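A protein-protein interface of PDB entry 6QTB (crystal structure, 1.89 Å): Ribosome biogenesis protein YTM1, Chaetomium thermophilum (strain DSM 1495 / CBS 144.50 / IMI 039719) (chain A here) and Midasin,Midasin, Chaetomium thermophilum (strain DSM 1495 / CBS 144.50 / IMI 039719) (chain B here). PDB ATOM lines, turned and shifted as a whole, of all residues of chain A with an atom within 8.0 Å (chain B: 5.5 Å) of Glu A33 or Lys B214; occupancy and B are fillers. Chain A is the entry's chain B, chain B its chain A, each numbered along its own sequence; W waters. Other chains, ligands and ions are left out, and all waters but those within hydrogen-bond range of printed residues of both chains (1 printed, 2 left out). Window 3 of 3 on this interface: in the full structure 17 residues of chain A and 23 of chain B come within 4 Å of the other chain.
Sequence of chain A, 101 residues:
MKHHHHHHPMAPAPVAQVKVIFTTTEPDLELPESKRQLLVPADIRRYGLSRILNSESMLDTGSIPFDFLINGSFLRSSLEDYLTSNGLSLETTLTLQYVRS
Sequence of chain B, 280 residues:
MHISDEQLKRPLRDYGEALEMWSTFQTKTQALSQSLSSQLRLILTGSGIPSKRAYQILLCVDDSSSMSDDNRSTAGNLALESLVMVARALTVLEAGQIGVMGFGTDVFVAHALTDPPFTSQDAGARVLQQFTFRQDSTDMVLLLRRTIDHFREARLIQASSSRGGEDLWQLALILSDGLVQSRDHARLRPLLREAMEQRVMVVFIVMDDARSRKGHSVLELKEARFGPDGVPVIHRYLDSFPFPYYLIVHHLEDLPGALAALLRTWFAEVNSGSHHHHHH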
ATOM      1  N   ILE A  21       8.971   5.784  -1.557  1.00  0.00           N
ATOM      2  CA  ILE A  21      10.141   5.376  -0.768  1.00  0.00           C
ATOM      3  C   ILE A  21      10.533   3.992  -1.210  1.00  0.00           C
ATOM      4  O   ILE A  21       9.730   3.063  -1.104  1.00  0.00           O
ATOM      5  CB  ILE A  21       9.886   5.398   0.754  1.00  0.00           C
ATOM      6  CG1 ILE A  21       9.609   6.820   1.215  1.00  0.00           C
ATOM      7  CG2 ILE A  21      11.139   4.874   1.507  1.00  0.00           C
ATOM      8  CD1 ILE A  21       8.988   6.852   2.609  1.00  0.00           C
ATOM      9  N   PHE A  22      11.782   3.839  -1.690  1.00  0.00           N
ATOM     10  CA  PHE A  22      12.238   2.537  -2.149  1.00  0.00           C
ATOM     11  C   PHE A  22      12.764   1.744  -0.978  1.00  0.00           C
ATOM     12  O   PHE A  22      13.463   2.280  -0.099  1.00  0.00           O
ATOM     13  CB  PHE A  22      13.358   2.696  -3.198  1.00  0.00           C
ATOM     14  CG  PHE A  22      12.860   3.173  -4.547  1.00  0.00           C
ATOM     15  CD1 PHE A  22      11.944   2.425  -5.267  1.00  0.00           C
ATOM     16  CD2 PHE A  22      13.286   4.379  -5.055  1.00  0.00           C
ATOM     17  CE1 PHE A  22      11.510   2.864  -6.506  1.00  0.00           C
ATOM     18  CE2 PHE A  22      12.864   4.841  -6.272  1.00  0.00           C
ATOM     19  CZ  PHE A  22      11.950   4.095  -7.011  1.00  0.00           C
ATOM     20  N   GLU A  30      20.839  -2.658  -1.858  1.00  0.00           N
ATOM     21  CA  GLU A  30      20.352  -1.524  -1.084  1.00  0.00           C
ATOM     22  C   GLU A  30      20.880  -0.207  -1.660  1.00  0.00           C
ATOM     23  O   GLU A  30      22.020  -0.123  -2.129  1.00  0.00           O
ATOM     24  CB  GLU A  30      20.836  -1.650   0.363  1.00  0.00           C
ATOM     25  CG  GLU A  30      19.838  -2.155   1.364  1.00  0.00           C
ATOM     26  CD  GLU A  30      20.413  -2.133   2.795  1.00  0.00           C
ATOM     27  OE1 GLU A  30      21.607  -1.792   2.970  1.00  0.00           O
ATOM     28  OE2 GLU A  30      19.674  -2.497   3.738  1.00  0.00           O
ATOM     29  N   LEU A  31      20.071   0.832  -1.564  1.00  0.00           N
ATOM     30  CA  LEU A  31      20.462   2.198  -1.854  1.00  0.00           C
ATOM     31  C   LEU A  31      20.971   2.838  -0.571  1.00  0.00           C
ATOM     32  O   LEU A  31      20.488   2.511   0.508  1.00  0.00           O
ATOM     33  CB  LEU A  31      19.250   3.008  -2.324  1.00  0.00           C
ATOM     34  CG  LEU A  31      18.688   2.691  -3.715  1.00  0.00           C
ATOM     35  CD1 LEU A  31      17.239   3.168  -3.750  1.00  0.00           C
ATOM     36  CD2 LEU A  31      19.541   3.384  -4.767  1.00  0.00           C
ATOM     37  N   PRO A  32      21.845   3.832  -0.649  1.00  0.00           N
ATOM     38  CA  PRO A  32      22.108   4.637   0.556  1.00  0.00           C
ATOM     39  C   PRO A  32      20.813   5.315   0.986  1.00  0.00           C
ATOM     40  O   PRO A  32      19.974   5.669   0.146  1.00  0.00           O
ATOM     41  CB  PRO A  32      23.151   5.662   0.093  1.00  0.00           C
ATOM     42  CG  PRO A  32      23.023   5.679  -1.436  1.00  0.00           C
ATOM     43  CD  PRO A  32      22.600   4.286  -1.839  1.00  0.00           C
ATOM     44  N   GLU A  33      20.686   5.526   2.309  1.00  0.00           N
ATOM     45  CA  GLU A  33      19.478   6.106   2.882  1.00  0.00           C
ATOM     46  C   GLU A  33      19.104   7.391   2.167  1.00  0.00           C
ATOM     47  O   GLU A  33      17.921   7.685   1.970  1.00  0.00           O
ATOM     48  CB  GLU A  33      19.717   6.416   4.371  1.00  0.00           C
ATOM     49  CG  GLU A  33      19.339   5.335   5.370  1.00  0.00           C
ATOM     50  CD  GLU A  33      19.791   5.693   6.804  1.00  0.00           C
ATOM     51  OE1 GLU A  33      21.002   5.607   7.109  1.00  0.00           O
ATOM     52  OE2 GLU A  33      18.932   6.104   7.623  1.00  0.00           O
ATOM     53  N   SER A  34      20.104   8.171   1.769  1.00  0.00           N
ATOM     54  CA  SER A  34      19.896   9.459   1.121  1.00  0.00           C
ATOM     55  C   SER A  34      19.267   9.357  -0.261  1.00  0.00           C
ATOM     56  O   SER A  34      18.860  10.394  -0.809  1.00  0.00           O
ATOM     57  CB  SER A  34      21.246  10.184   1.041  1.00  0.00           C
ATOM     58  OG  SER A  34      22.095   9.581   0.058  1.00  0.00           O
ATOM     59  N   LYS A  35      19.250   8.164  -0.885  1.00  0.00           N
ATOM     60  CA  LYS A  35      18.645   8.030  -2.212  1.00  0.00           C
ATOM     61  C   LYS A  35      17.323   7.264  -2.209  1.00  0.00           C
ATOM     62  O   LYS A  35      16.815   6.963  -3.295  1.00  0.00           O
ATOM     63  CB  LYS A  35      19.605   7.334  -3.178  1.00  0.00           C
ATOM     64  CG  LYS A  35      20.950   8.155  -3.440  1.00  0.00           C
ATOM     65  CD  LYS A  35      21.911   7.265  -4.242  1.00  0.00           C
ATOM     66  CE  LYS A  35      23.388   7.750  -4.252  1.00  0.00           C
ATOM     67  NZ  LYS A  35      23.552   8.777  -5.270  1.00  0.00           N
ATOM     68  N   ARG A  36      16.759   6.927  -1.038  1.00  0.00           N
ATOM     69  CA  ARG A  36      15.561   6.086  -1.056  1.00  0.00           C
ATOM     70  C   ARG A  36      14.244   6.854  -1.225  1.00  0.00           C
ATOM     71  O   ARG A  36      13.229   6.235  -1.600  1.00  0.00           O
ATOM     72  CB  ARG A  36      15.465   5.299   0.238  1.00  0.00           C
ATOM     73  CG  ARG A  36      16.646   4.246   0.325  1.00  0.00           C
ATOM     74  CD  ARG A  36      16.638   3.488   1.645  1.00  0.00           C
ATOM     75  NE  ARG A  36      17.955   2.883   1.853  1.00  0.00           N
ATOM     76  CZ  ARG A  36      18.322   2.250   2.967  1.00  0.00           C
ATOM     77  NH1 ARG A  36      17.469   2.178   3.987  1.00  0.00           N
ATOM     78  NH2 ARG A  36      19.548   1.718   3.063  1.00  0.00           N
ATOM     79  N   GLN A  37      14.228   8.141  -0.946  1.00  0.00           N
ATOM     80  CA  GLN A  37      12.984   8.914  -1.050  1.00  0.00           C
ATOM     81  C   GLN A  37      13.001   9.731  -2.315  1.00  0.00           C
ATOM     82  O   GLN A  37      13.891  10.580  -2.474  1.00  0.00           O
ATOM     83  CB  GLN A  37      12.822   9.883   0.120  1.00  0.00           C
ATOM     84  CG  GLN A  37      12.914   9.433   1.487  1.00  0.00           C
ATOM     85  CD  GLN A  37      13.012  10.716   2.333  1.00  0.00           C
ATOM     86  OE1 GLN A  37      14.118  11.215   2.572  1.00  0.00           O
ATOM     87  NE2 GLN A  37      11.853  11.347   2.615  1.00  0.00           N
ATOM     88  N   SER B 212      10.547  10.768  13.343  1.00  0.00           N
ATOM     89  CA  SER B 212       9.637  10.030  12.472  1.00  0.00           C
ATOM     90  C   SER B 212      10.182   8.658  12.092  1.00  0.00           C
ATOM     91  O   SER B 212       9.660   7.624  12.534  1.00  0.00           O
ATOM     92  CB  SER B 212       9.355  10.833  11.199  1.00  0.00           C
ATOM     93  OG  SER B 212       8.554  10.076  10.303  1.00  0.00           O
ATOM     94  N   ARG B 213      11.277   8.630  11.330  1.00  0.00           N
ATOM     95  CA  ARG B 213      11.973   7.379  11.036  1.00  0.00           C
ATOM     96  C   ARG B 213      13.438   7.660  10.755  1.00  0.00           C
ATOM     97  O   ARG B 213      13.828   8.783  10.414  1.00  0.00           O
ATOM     98  CB  ARG B 213      11.378   6.615   9.845  1.00  0.00           C
ATOM     99  CG  ARG B 213      10.083   5.932  10.152  1.00  0.00           C
ATOM    100  CD  ARG B 213       8.873   6.763   9.712  1.00  0.00           C
ATOM    101  NE  ARG B 213       8.569   6.464   8.312  1.00  0.00           N
ATOM    102  CZ  ARG B 213       7.828   5.416   7.945  1.00  0.00           C
ATOM    103  NH1 ARG B 213       7.348   4.609   8.882  1.00  0.00           N
ATOM    104  NH2 ARG B 213       7.584   5.152   6.658  1.00  0.00           N
ATOM    105  N   LYS B 214      14.240   6.607  10.880  1.00  0.00           N
ATOM    106  CA  LYS B 214      15.647   6.707  10.527  1.00  0.00           C
ATOM    107  C   LYS B 214      15.708   6.979   9.022  1.00  0.00           C
ATOM    108  O   LYS B 214      15.114   6.226   8.238  1.00  0.00           O
ATOM    109  CB  LYS B 214      16.372   5.391  10.821  1.00  0.00           C
ATOM    110  CG  LYS B 214      17.898   5.484  10.946  1.00  0.00           C
ATOM    111  CD  LYS B 214      18.496   4.113  11.053  1.00  0.00           C
ATOM    112  CE  LYS B 214      19.553   4.127   9.894  1.00  0.00           C
ATOM    113  NZ  LYS B 214      20.014   2.723   9.545  1.00  0.00           N
ATOM    114  N   GLY B 215      16.388   8.055   8.616  1.00  0.00           N
ATOM    115  CA  GLY B 215      16.668   8.270   7.200  1.00  0.00           C
ATOM    116  C   GLY B 215      15.549   8.788   6.313  1.00  0.00           C
ATOM    117  O   GLY B 215      15.527   8.457   5.112  1.00  0.00           O
ATOM    118  N   HIS B 216      14.607   9.575   6.855  1.00  0.00           N
ATOM    119  CA  HIS B 216      13.488  10.078   6.056  1.00  0.00           C
ATOM    120  C   HIS B 216      13.288  11.586   6.218  1.00  0.00           C
ATOM    121  O   HIS B 216      12.171  12.053   6.465  1.00  0.00           O
ATOM    122  CB  HIS B 216      12.196   9.362   6.394  1.00  0.00           C
ATOM    123  CG  HIS B 216      12.108   7.974   5.840  1.00  0.00           C
ATOM    124  ND1 HIS B 216      11.430   6.959   6.482  1.00  0.00           N
ATOM    125  CD2 HIS B 216      12.621   7.433   4.708  1.00  0.00           C
ATOM    126  CE1 HIS B 216      11.520   5.854   5.764  1.00  0.00           C
ATOM    127  NE2 HIS B 216      12.240   6.112   4.684  1.00  0.00           N
ATOM    128  N   GLU B 220      16.807  15.161   2.334  1.00  0.00           N
ATOM    129  CA  GLU B 220      17.314  14.148   1.395  1.00  0.00           C
ATOM    130  C   GLU B 220      16.284  13.717   0.370  1.00  0.00           C
ATOM    131  O   GLU B 220      16.546  12.760  -0.397  1.00  0.00           O
ATOM    132  CB  GLU B 220      17.777  12.900   2.155  1.00  0.00           C
ATOM    133  CG  GLU B 220      18.497  13.150   3.453  1.00  0.00           C
ATOM    134  CD  GLU B 220      19.983  13.160   3.263  1.00  0.00           C
ATOM    135  OE1 GLU B 220      20.441  13.651   2.198  1.00  0.00           O
ATOM    136  OE2 GLU B 220      20.689  12.634   4.157  1.00  0.00           O
HETATM  137  O   HOH W   1      14.842   4.142   4.495  1.00  0.00           O
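Printed residues of chain B within 4 Å of Gln A37: His B216 (3.7 Å) and Glu B220 (3.97 Å).
Lys B214 touches just one residue of chain A: Glu A33.
Printed residues of chain A within 4 Å of His B216: Ile A21 (3.6 Å) and Gln A37 (3.7 Å).
Printed residues of chain A within 4 Å of Glu B220: Ser A34 (3.3 Å) and Gln A37 (3.97 Å).
The nearest residue of chain A that does not touch Lys B214 is Arg A36 (6.1 Å).
The nearest printed residue of chain A that does not touch His B216 is Arg A36 (5.6 Å).
The guanidinium group of Arg B213 sits close to a ring nitrogen (ND1) of His B216 (3.4 Å).
Hydrophobic or aromatic side chains of chain A that line the printed part of chain B: Ile A21.
Of the 6 printed residues of chain B, 4 touch a printed residue of chain A.
Hydrophobic or aromatic side chains of chain B that line the printed part of chain A: His B216.
Along chain B the printed residues that touch a printed residue of chain A span positions 214 to 220.
Among the printed residues, 6 pairs touch across the chains.
Among the printed residues, Asp or Glu carboxylates within 4 Å of a Lys or Arg side-chain nitrogen of the other chain: Glu A33 with Lys B214 (3.9 Å).
Water W1 lies within hydrogen-bond range of NE2 of His B216 and NH1 of Arg A36.
The backbone carbonyl oxygen (O) of Ser A34 lies close to the backbone carbonyl oxygen (O) of Glu B220 (3.3 Å).
N of Gly B215 lies close to OE2 of Glu A33 (3.4 Å).
NZ of Lys B214 is in salt-bridge range of OE1 of Glu A33.
Among the printed residues, pairs that only touch across the chains: Ile A21 with His B216 (3.6 Å), Gln A37 with His B216 (3.7 Å) and Gln A37 with Glu B220 (3.97 Å).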
